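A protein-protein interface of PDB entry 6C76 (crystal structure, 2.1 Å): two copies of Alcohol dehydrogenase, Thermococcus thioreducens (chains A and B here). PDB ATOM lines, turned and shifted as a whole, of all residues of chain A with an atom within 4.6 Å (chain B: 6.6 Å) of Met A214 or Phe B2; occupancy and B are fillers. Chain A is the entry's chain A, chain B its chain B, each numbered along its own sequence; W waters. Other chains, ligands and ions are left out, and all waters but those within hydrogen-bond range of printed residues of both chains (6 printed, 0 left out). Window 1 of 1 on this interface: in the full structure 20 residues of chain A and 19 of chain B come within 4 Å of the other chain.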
ATOM      1  N   LEU A   4      -8.685   6.014   5.463  1.00  0.00           N
ATOM      2  CA  LEU A   4      -8.910   7.023   4.457  1.00  0.00           C
ATOM      3  C   LEU A   4      -8.217   8.315   4.877  1.00  0.00           C
ATOM      4  O   LEU A   4      -8.598   8.948   5.861  1.00  0.00           O
ATOM      5  CB  LEU A   4     -10.407   7.259   4.293  1.00  0.00           C
ATOM      6  CG  LEU A   4     -10.824   8.327   3.284  1.00  0.00           C
ATOM      7  CD1 LEU A   4     -10.510   7.913   1.858  1.00  0.00           C
ATOM      8  CD2 LEU A   4     -12.308   8.581   3.438  1.00  0.00           C
ATOM      9  N   THR A   6      -7.810  10.915   2.782  1.00  0.00           N
ATOM     10  CA  THR A   6      -8.385  11.993   2.035  1.00  0.00           C
ATOM     11  C   THR A   6      -9.675  12.495   2.646  1.00  0.00           C
ATOM     12  O   THR A   6     -10.617  11.735   2.856  1.00  0.00           O
ATOM     13  CB  THR A   6      -8.676  11.533   0.605  1.00  0.00           C
ATOM     14  OG1 THR A   6      -7.492  10.948   0.049  1.00  0.00           O
ATOM     15  CG2 THR A   6      -9.118  12.700  -0.246  1.00  0.00           C
ATOM     16  N   ARG A   7      -9.798  13.810   2.654  1.00  0.00           N
ATOM     17  CA  ARG A   7     -11.002  14.482   3.093  1.00  0.00           C
ATOM     18  C   ARG A   7     -11.822  14.812   1.855  1.00  0.00           C
ATOM     19  O   ARG A   7     -11.299  15.377   0.901  1.00  0.00           O
ATOM     20  CB  ARG A   7     -10.609  15.756   3.839  1.00  0.00           C
ATOM     21  CG  ARG A   7     -11.713  16.413   4.635  1.00  0.00           C
ATOM     22  CD  ARG A   7     -11.132  17.199   5.804  1.00  0.00           C
ATOM     23  NE  ARG A   7      -9.979  17.995   5.391  1.00  0.00           N
ATOM     24  CZ  ARG A   7     -10.060  19.116   4.676  1.00  0.00           C
ATOM     25  NH1 ARG A   7     -11.243  19.656   4.399  1.00  0.00           N
ATOM     26  NH2 ARG A   7      -8.952  19.711   4.255  1.00  0.00           N
ATOM     27  N   ILE A   8     -13.029  14.259   1.792  1.00  0.00           N
ATOM     28  CA  ILE A   8     -13.895  14.418   0.640  1.00  0.00           C
ATOM     29  C   ILE A   8     -14.924  15.542   0.789  1.00  0.00           C
ATOM     30  O   ILE A   8     -15.738  15.553   1.715  1.00  0.00           O
ATOM     31  CB  ILE A   8     -14.637  13.116   0.332  1.00  0.00           C
ATOM     32  CG1 ILE A   8     -13.634  12.004   0.037  1.00  0.00           C
ATOM     33  CG2 ILE A   8     -15.567  13.317  -0.854  1.00  0.00           C
ATOM     34  CD1 ILE A   8     -14.237  10.619   0.113  1.00  0.00           C
ATOM     35  N   GLU A  10     -18.098  17.081  -1.400  1.00  0.00           N
ATOM     36  CA  GLU A  10     -18.951  16.769  -2.544  1.00  0.00           C
ATOM     37  C   GLU A  10     -20.123  17.724  -2.629  1.00  0.00           C
ATOM     38  O   GLU A  10     -20.512  18.319  -1.627  1.00  0.00           O
ATOM     39  CB  GLU A  10     -19.466  15.332  -2.470  1.00  0.00           C
ATOM     40  CG  GLU A  10     -20.765  15.169  -1.696  1.00  0.00           C
ATOM     41  CD  GLU A  10     -20.520  14.907  -0.232  1.00  0.00           C
ATOM     42  OE1 GLU A  10     -21.264  14.109   0.354  1.00  0.00           O
ATOM     43  OE2 GLU A  10     -19.500  15.384   0.292  1.00  0.00           O
ATOM     44  N   PHE A 210     -15.580  -3.193   5.674  1.00  0.00           N
ATOM     45  CA  PHE A 210     -15.616  -1.747   5.481  1.00  0.00           C
ATOM     46  C   PHE A 210     -15.424  -1.384   4.024  1.00  0.00           C
ATOM     47  O   PHE A 210     -16.168  -0.575   3.477  1.00  0.00           O
ATOM     48  CB  PHE A 210     -14.556  -1.062   6.332  1.00  0.00           C
ATOM     49  CG  PHE A 210     -14.691  -1.353   7.796  1.00  0.00           C
ATOM     50  CD1 PHE A 210     -15.579  -0.635   8.574  1.00  0.00           C
ATOM     51  CD2 PHE A 210     -14.035  -2.430   8.362  1.00  0.00           C
ATOM     52  CE1 PHE A 210     -15.751  -0.932   9.915  1.00  0.00           C
ATOM     53  CE2 PHE A 210     -14.233  -2.757   9.689  1.00  0.00           C
ATOM     54  CZ  PHE A 210     -15.117  -2.028  10.460  1.00  0.00           C
ATOM     55  N   SER A 211     -14.508  -2.066   3.360  1.00  0.00           N
ATOM     56  CA  SER A 211     -14.306  -1.816   1.950  1.00  0.00           C
ATOM     57  C   SER A 211     -15.432  -2.438   1.141  1.00  0.00           C
ATOM     58  O   SER A 211     -15.865  -1.858   0.147  1.00  0.00           O
ATOM     59  CB  SER A 211     -12.943  -2.345   1.494  1.00  0.00           C
ATOM     60  OG  SER A 211     -12.872  -3.754   1.596  1.00  0.00           O
ATOM     61  N   ASP A 212     -16.013  -3.514   1.674  1.00  0.00           N
ATOM     62  CA  ASP A 212     -17.159  -4.168   1.056  1.00  0.00           C
ATOM     63  C   ASP A 212     -18.346  -3.226   0.914  1.00  0.00           C
ATOM     64  O   ASP A 212     -19.003  -3.200  -0.113  1.00  0.00           O
ATOM     65  CB  ASP A 212     -17.576  -5.397   1.879  1.00  0.00           C
ATOM     66  CG  ASP A 212     -16.732  -6.637   1.566  1.00  0.00           C
ATOM     67  OD1 ASP A 212     -15.799  -6.552   0.743  1.00  0.00           O
ATOM     68  OD2 ASP A 212     -16.905  -7.659   2.258  1.00  0.00           O
ATOM     69  N   ALA A 213     -18.630  -2.469   1.964  1.00  0.00           N
ATOM     70  CA  ALA A 213     -19.731  -1.504   1.958  1.00  0.00           C
ATOM     71  C   ALA A 213     -19.648  -0.517   0.785  1.00  0.00           C
ATOM     72  O   ALA A 213     -20.672  -0.067   0.252  1.00  0.00           O
ATOM     73  CB  ALA A 213     -19.727  -0.741   3.273  1.00  0.00           C
ATOM     74  N   MET A 214     -18.453   0.023   0.595  1.00  0.00           N
ATOM     75  CA  MET A 214     -18.210   0.997  -0.459  1.00  0.00           C
ATOM     76  C   MET A 214     -18.279   0.302  -1.808  1.00  0.00           C
ATOM     77  O   MET A 214     -18.901   0.805  -2.747  1.00  0.00           O
ATOM     78  CB  MET A 214     -16.835   1.635  -0.268  1.00  0.00           C
ATOM     79  CG  MET A 214     -16.747   2.466   1.002  1.00  0.00           C
ATOM     80  SD  MET A 214     -17.709   3.975   0.805  1.00  0.00           S
ATOM     81  CE  MET A 214     -17.422   4.819   2.354  1.00  0.00           C
ATOM     82  N   ALA A 215     -17.693  -0.886  -1.881  1.00  0.00           N
ATOM     83  CA  ALA A 215     -17.628  -1.618  -3.150  1.00  0.00           C
ATOM     84  C   ALA A 215     -19.043  -1.933  -3.634  1.00  0.00           C
ATOM     85  O   ALA A 215     -19.395  -1.668  -4.782  1.00  0.00           O
ATOM     86  CB  ALA A 215     -16.826  -2.902  -2.981  1.00  0.00           C
ATOM     87  N   ILE A 216     -19.879  -2.420  -2.726  1.00  0.00           N
ATOM     88  CA  ILE A 216     -21.212  -2.875  -3.103  1.00  0.00           C
ATOM     89  C   ILE A 216     -22.097  -1.712  -3.565  1.00  0.00           C
ATOM     90  O   ILE A 216     -22.748  -1.786  -4.597  1.00  0.00           O
ATOM     91  CB  ILE A 216     -21.876  -3.642  -1.944  1.00  0.00           C
ATOM     92  CG1 ILE A 216     -21.535  -5.120  -2.061  1.00  0.00           C
ATOM     93  CG2 ILE A 216     -23.390  -3.486  -1.983  1.00  0.00           C
ATOM     94  CD1 ILE A 216     -22.177  -5.785  -3.263  1.00  0.00           C
ATOM     95  N   LYS A 217     -22.014  -0.588  -2.874  1.00  0.00           N
ATOM     96  CA  LYS A 217     -22.802   0.578  -3.255  1.00  0.00           C
ATOM     97  C   LYS A 217     -22.395   1.147  -4.621  1.00  0.00           C
ATOM     98  O   LYS A 217     -23.232   1.639  -5.376  1.00  0.00           O
ATOM     99  CB  LYS A 217     -22.688   1.644  -2.170  1.00  0.00           C
ATOM    100  CG  LYS A 217     -23.563   2.863  -2.388  1.00  0.00           C
ATOM    101  CD  LYS A 217     -25.006   2.619  -1.995  1.00  0.00           C
ATOM    102  CE  LYS A 217     -25.814   3.916  -2.035  1.00  0.00           C
ATOM    103  NZ  LYS A 217     -25.019   5.055  -1.499  1.00  0.00           N
ATOM    104  N   ALA A 218     -21.096   1.181  -4.884  1.00  0.00           N
ATOM    105  CA  ALA A 218     -20.597   1.588  -6.184  1.00  0.00           C
ATOM    106  C   ALA A 218     -21.134   0.702  -7.297  1.00  0.00           C
ATOM    107  O   ALA A 218     -21.499   1.199  -8.351  1.00  0.00           O
ATOM    108  CB  ALA A 218     -19.088   1.558  -6.189  1.00  0.00           C
ATOM    109  N   MET A 246     -16.365   6.111  -4.302  1.00  0.00           N
ATOM    110  CA  MET A 246     -16.675   4.959  -3.444  1.00  0.00           C
ATOM    111  C   MET A 246     -15.832   3.751  -3.821  1.00  0.00           C
ATOM    112  O   MET A 246     -15.295   3.079  -2.950  1.00  0.00           O
ATOM    113  CB  MET A 246     -18.149   4.579  -3.558  1.00  0.00           C
ATOM    114  CG  MET A 246     -19.081   5.436  -2.720  1.00  0.00           C
ATOM    115  SD  MET A 246     -20.810   4.920  -2.867  1.00  0.00           S
ATOM    116  CE  MET A 246     -21.578   6.503  -2.568  1.00  0.00           C
ATOM    117  N   ILE A 249     -12.259   4.242  -2.745  1.00  0.00           N
ATOM    118  CA  ILE A 249     -12.056   4.022  -1.329  1.00  0.00           C
ATOM    119  C   ILE A 249     -11.962   2.537  -1.064  1.00  0.00           C
ATOM    120  O   ILE A 249     -11.157   2.092  -0.243  1.00  0.00           O
ATOM    121  CB  ILE A 249     -13.212   4.592  -0.497  1.00  0.00           C
ATOM    122  CG1 ILE A 249     -13.304   6.105  -0.665  1.00  0.00           C
ATOM    123  CG2 ILE A 249     -13.037   4.235   0.969  1.00  0.00           C
ATOM    124  CD1 ILE A 249     -14.531   6.705  -0.007  1.00  0.00           C
ATOM    125  N   ALA A 250     -12.825   1.764  -1.709  1.00  0.00           N
ATOM    126  CA  ALA A 250     -12.754   0.309  -1.578  1.00  0.00           C
ATOM    127  C   ALA A 250     -11.396  -0.221  -2.007  1.00  0.00           C
ATOM    128  O   ALA A 250     -10.830  -1.066  -1.328  1.00  0.00           O
ATOM    129  CB  ALA A 250     -13.854  -0.363  -2.382  1.00  0.00           C
ATOM    130  N   MET B   1     -19.963  16.195   2.685  1.00  0.00           N
ATOM    131  CA  MET B   1     -18.585  16.077   3.213  1.00  0.00           C
ATOM    132  C   MET B   1     -18.419  14.726   3.887  1.00  0.00           C
ATOM    133  O   MET B   1     -19.359  14.191   4.470  1.00  0.00           O
ATOM    134  CB  MET B   1     -18.305  17.198   4.208  1.00  0.00           C
ATOM    135  CG  MET B   1     -16.917  17.133   4.820  1.00  0.00           C
ATOM    136  SD  MET B   1     -16.183  18.758   5.077  1.00  0.00           S
ATOM    137  CE  MET B   1     -14.515  18.447   4.501  1.00  0.00           C
ATOM    138  N   PHE B   2     -17.264  14.111   3.693  1.00  0.00           N
ATOM    139  CA  PHE B   2     -17.016  12.817   4.275  1.00  0.00           C
ATOM    140  C   PHE B   2     -15.571  12.701   4.681  1.00  0.00           C
ATOM    141  O   PHE B   2     -14.673  12.917   3.875  1.00  0.00           O
ATOM    142  CB  PHE B   2     -17.360  11.707   3.292  1.00  0.00           C
ATOM    143  CG  PHE B   2     -17.235  10.332   3.878  1.00  0.00           C
ATOM    144  CD1 PHE B   2     -18.208   9.846   4.745  1.00  0.00           C
ATOM    145  CD2 PHE B   2     -16.115   9.551   3.625  1.00  0.00           C
ATOM    146  CE1 PHE B   2     -18.110   8.574   5.279  1.00  0.00           C
ATOM    147  CE2 PHE B   2     -15.993   8.293   4.186  1.00  0.00           C
ATOM    148  CZ  PHE B   2     -17.019   7.783   4.966  1.00  0.00           C
ATOM    149  N   TRP B   3     -15.340  12.330   5.930  1.00  0.00           N
ATOM    150  CA  TRP B   3     -14.016  11.924   6.304  1.00  0.00           C
ATOM    151  C   TRP B   3     -13.930  10.992   7.484  1.00  0.00           C
ATOM    152  O   TRP B   3     -14.931  10.672   8.130  1.00  0.00           O
ATOM    153  CB  TRP B   3     -13.138  13.138   6.525  1.00  0.00           C
ATOM    154  CG  TRP B   3     -13.582  14.041   7.584  1.00  0.00           C
ATOM    155  CD1 TRP B   3     -13.899  15.357   7.426  1.00  0.00           C
ATOM    156  CD2 TRP B   3     -13.419  13.837   8.994  1.00  0.00           C
ATOM    157  NE1 TRP B   3     -13.942  15.982   8.645  1.00  0.00           N
ATOM    158  CE2 TRP B   3     -13.676  15.064   9.626  1.00  0.00           C
ATOM    159  CE3 TRP B   3     -13.085  12.730   9.784  1.00  0.00           C
ATOM    160  CZ2 TRP B   3     -13.674  15.204  11.013  1.00  0.00           C
ATOM    161  CZ3 TRP B   3     -13.072  12.873  11.163  1.00  0.00           C
ATOM    162  CH2 TRP B   3     -13.349  14.104  11.761  1.00  0.00           C
ATOM    163  N   LEU B   4     -12.711  10.525   7.719  1.00  0.00           N
ATOM    164  CA  LEU B   4     -12.434   9.550   8.754  1.00  0.00           C
ATOM    165  C   LEU B   4     -10.993   9.709   9.214  1.00  0.00           C
ATOM    166  O   LEU B   4     -10.055   9.333   8.508  1.00  0.00           O
ATOM    167  CB  LEU B   4     -12.675   8.137   8.225  1.00  0.00           C
ATOM    168  CG  LEU B   4     -12.484   6.978   9.204  1.00  0.00           C
ATOM    169  CD1 LEU B   4     -13.535   6.963  10.295  1.00  0.00           C
ATOM    170  CD2 LEU B   4     -12.539   5.671   8.447  1.00  0.00           C
ATOM    171  N   SER B 208     -24.872  11.739   3.123  1.00  0.00           N
ATOM    172  CA  SER B 208     -24.287  11.637   1.800  1.00  0.00           C
ATOM    173  C   SER B 208     -24.195  10.180   1.376  1.00  0.00           C
ATOM    174  O   SER B 208     -24.276   9.277   2.215  1.00  0.00           O
ATOM    175  CB  SER B 208     -22.892  12.248   1.808  1.00  0.00           C
ATOM    176  OG  SER B 208     -21.973  11.395   2.458  1.00  0.00           O
ATOM    177  N   PRO B 209     -23.936   9.949   0.079  1.00  0.00           N
ATOM    178  CA  PRO B 209     -23.801   8.603  -0.458  1.00  0.00           C
ATOM    179  C   PRO B 209     -22.719   7.832   0.269  1.00  0.00           C
ATOM    180  O   PRO B 209     -22.869   6.632   0.508  1.00  0.00           O
ATOM    181  CB  PRO B 209     -23.389   8.839  -1.914  1.00  0.00           C
ATOM    182  CG  PRO B 209     -23.781  10.241  -2.204  1.00  0.00           C
ATOM    183  CD  PRO B 209     -23.600  10.971  -0.920  1.00  0.00           C
ATOM    184  N   PHE B 210     -21.701   8.552   0.734  1.00  0.00           N
ATOM    185  CA  PHE B 210     -20.598   7.937   1.467  1.00  0.00           C
ATOM    186  C   PHE B 210     -21.027   7.418   2.839  1.00  0.00           C
ATOM    187  O   PHE B 210     -20.781   6.265   3.169  1.00  0.00           O
ATOM    188  CB  PHE B 210     -19.436   8.926   1.597  1.00  0.00           C
ATOM    189  CG  PHE B 210     -18.869   9.346   0.281  1.00  0.00           C
ATOM    190  CD1 PHE B 210     -18.114   8.463  -0.467  1.00  0.00           C
ATOM    191  CD2 PHE B 210     -19.265  10.530  -0.300  1.00  0.00           C
ATOM    192  CE1 PHE B 210     -17.706   8.790  -1.747  1.00  0.00           C
ATOM    193  CE2 PHE B 210     -18.835  10.876  -1.565  1.00  0.00           C
ATOM    194  CZ  PHE B 210     -18.113   9.974  -2.316  1.00  0.00           C
ATOM    195  N   SER B 211     -21.720   8.238   3.618  1.00  0.00           N
ATOM    196  CA  SER B 211     -22.231   7.753   4.896  1.00  0.00           C
ATOM    197  C   SER B 211     -23.352   6.745   4.688  1.00  0.00           C
ATOM    198  O   SER B 211     -23.410   5.735   5.386  1.00  0.00           O
ATOM    199  CB  SER B 211     -22.697   8.897   5.793  1.00  0.00           C
ATOM    200  OG  SER B 211     -23.659   9.698   5.143  1.00  0.00           O
ATOM    201  N   ASP B 212     -24.146   6.954   3.641  1.00  0.00           N
ATOM    202  CA  ASP B 212     -25.218   6.030   3.296  1.00  0.00           C
ATOM    203  C   ASP B 212     -24.700   4.630   3.112  1.00  0.00           C
ATOM    204  O   ASP B 212     -25.318   3.685   3.580  1.00  0.00           O
ATOM    205  CB  ASP B 212     -25.921   6.477   2.025  1.00  0.00           C
ATOM    206  CG  ASP B 212     -26.820   7.662   2.253  1.00  0.00           C
ATOM    207  OD1 ASP B 212     -26.959   8.091   3.424  1.00  0.00           O
ATOM    208  OD2 ASP B 212     -27.411   8.149   1.272  1.00  0.00           O
ATOM    209  N   ALA B 213     -23.569   4.485   2.426  1.00  0.00           N
ATOM    210  CA  ALA B 213     -23.014   3.153   2.181  1.00  0.00           C
ATOM    211  C   ALA B 213     -22.767   2.418   3.492  1.00  0.00           C
ATOM    212  O   ALA B 213     -22.822   1.181   3.552  1.00  0.00           O
ATOM    213  CB  ALA B 213     -21.717   3.251   1.389  1.00  0.00           C
ATOM    214  N   MET B 214     -22.254   3.159   4.465  1.00  0.00           N
ATOM    215  CA  MET B 214     -21.910   2.569   5.740  1.00  0.00           C
ATOM    216  C   MET B 214     -23.179   2.273   6.548  1.00  0.00           C
ATOM    217  O   MET B 214     -23.339   1.185   7.087  1.00  0.00           O
ATOM    218  CB  MET B 214     -20.978   3.506   6.512  1.00  0.00           C
ATOM    219  CG  MET B 214     -19.585   3.637   5.906  1.00  0.00           C
ATOM    220  SD  MET B 214     -18.616   2.126   6.079  1.00  0.00           S
ATOM    221  CE  MET B 214     -17.004   2.682   5.527  1.00  0.00           C
ATOM    222  N   ILE B 249     -19.149   5.322  11.815  1.00  0.00           N
ATOM    223  CA  ILE B 249     -18.594   6.095  10.722  1.00  0.00           C
ATOM    224  C   ILE B 249     -19.688   6.884  10.028  1.00  0.00           C
ATOM    225  O   ILE B 249     -19.525   8.066   9.745  1.00  0.00           O
ATOM    226  CB  ILE B 249     -17.897   5.188   9.703  1.00  0.00           C
ATOM    227  CG1 ILE B 249     -16.722   4.484  10.369  1.00  0.00           C
ATOM    228  CG2 ILE B 249     -17.414   5.997   8.507  1.00  0.00           C
ATOM    229  CD1 ILE B 249     -16.090   3.427   9.496  1.00  0.00           C
ATOM    230  N   ALA B 250     -20.857   6.274   9.885  1.00  0.00           N
ATOM    231  CA  ALA B 250     -21.997   6.971   9.293  1.00  0.00           C
ATOM    232  C   ALA B 250     -22.435   8.179  10.113  1.00  0.00           C
ATOM    233  O   ALA B 250     -22.677   9.254   9.559  1.00  0.00           O
ATOM    234  CB  ALA B 250     -23.163   6.021   9.094  1.00  0.00           C
ATOM    235  N   ASN B 253     -20.304  11.250  10.236  1.00  0.00           N
ATOM    236  CA  ASN B 253     -20.426  12.151   9.101  1.00  0.00           C
ATOM    237  C   ASN B 253     -21.822  12.741   8.942  1.00  0.00           C
ATOM    238  O   ASN B 253     -21.963  13.914   8.650  1.00  0.00           O
ATOM    239  CB  ASN B 253     -19.976  11.452   7.826  1.00  0.00           C
ATOM    240  CG  ASN B 253     -18.473  11.340   7.745  1.00  0.00           C
ATOM    241  OD1 ASN B 253     -17.801  12.330   7.436  1.00  0.00           O
ATOM    242  ND2 ASN B 253     -17.944  10.277   8.340  1.00  0.00           N
HETATM  243  O   HOH W   1     -23.230  -0.369   1.371  1.00  0.00           O
HETATM  244  O   HOH W   2     -19.299  18.596   1.327  1.00  0.00           O
HETATM  245  O   HOH W   3     -27.660   6.363  -1.030  1.00  0.00           O
HETATM  246  O   HOH W   4      -8.835   6.810   8.367  1.00  0.00           O
HETATM  247  O   HOH W   5     -10.525  10.950   5.798  1.00  0.00           O
HETATM  248  O   HOH W   6     -22.096  18.301   1.108  1.00  0.00           O
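Among the printed residues, merely in contact across the chains: Glu A10 with Ser B208, Met A246 with Pro B209, Ile A8 with Met B1, Arg A7 with Met B1, Ala A213 with Ala B213, Arg A7 with Trp B3, Met A214 with Phe B210, Met A246 with Phe B210, Leu A4 with Phe B2, Met A214 with Met B214, Lys A217 with Asp B212, Phe A210 with Met B214, Met A214 with Phe B2 and Arg A7 with Phe B2.
Of the printed residues of chain B, Arg A7 touches Met B1, Phe B2 and Trp B3.
Of the printed residues of chain B, Glu A10 touches Met B1 and Ser B208.
Of chain B, only Phe B2 (3.97 Å), Phe B210 (3.7 Å) and Met B214 (3.8 Å) come within 4 Å of Met A214.
Phe B2 touches just these residues of chain A: Leu A4, Arg A7, Ile A8 and Met A214.
Of the printed residues of chain A, Asp B212 touches Lys A217 (3.9 Å).
Water W1 lies within hydrogen-bond range of the backbone carbonyl oxygen of Ala B213 (2.7 Å) and the backbone carbonyl oxygen of Ala A213 (2.8 Å).
Water W5 lies within hydrogen-bond range of O of Leu A4 (2.8 Å), N of Leu B4 (2.9 Å) and O of Thr A6 (3.0 Å).
Water W4 bridges the backbone carbonyl oxygen (O) of Leu B4 (2.8 Å) and the backbone NH (N) of Leu A4 (3.0 Å).
Water W2 lies within hydrogen-bond range of N of Met B1 (2.8 Å) and O of Glu A10 (3.2 Å).
Water W3 bridges OD2 of Asp B212 (2.9 Å) and NZ of Lys A217 (3.0 Å).
Water W6 lies within hydrogen-bond range of O of Glu A10 and N of Met B1.
Leu B4 touches its own counterpart, Leu A4.
Phe A210 touches Met B214, and with the chains exchanged Met A214 touches Phe B210.
Ala A213 touches its own counterpart, Ala B213.
Met B214 touches its own counterpart, Met A214.
8 positions are printed for both chains.
Of the 18 pairs that touch across the chains among the printed residues, 5 have their exchanged pair printed and touching as well.
Of the 17 printed residues of chain A, 9 touch a printed residue of chain B.
Hydrophobic or aromatic side chains of chain B within 4 Å of the printed part of chain A: Met B1, Phe B2, Trp B3, Pro B209, Phe B210, Ala B213 and Met B214.
Among the printed residues, 18 pairs touch across the chains.
Among the printed residues, no Asp or Glu carboxylate lies within 4 Å of a Lys or Arg side-chain nitrogen of the other chain.
O of Leu B4 sits close to O of Leu A4 (3.0 Å).
OE2 of Glu A10 is in hydrogen-bond range of N of Met B1 (2.6 Å).
The backbone carbonyl oxygen of Ile A8 lies within hydrogen-bond range of the backbone NH of Phe B2.
O of Pro B209 is in hydrogen-bond range of NZ of Lys A217 (3.3 Å).
O of Ser B208 sits at hydrogen-bond distance from OG of Ser B211 (3.0 Å).
N of Phe B210 sits close to OG of Ser B208, 3.3 Å away.
The backbone NH (N) of Trp B3 sits at hydrogen-bond distance from the side-chain amide oxygen (OD1) of Asn B253 (2.9 Å).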
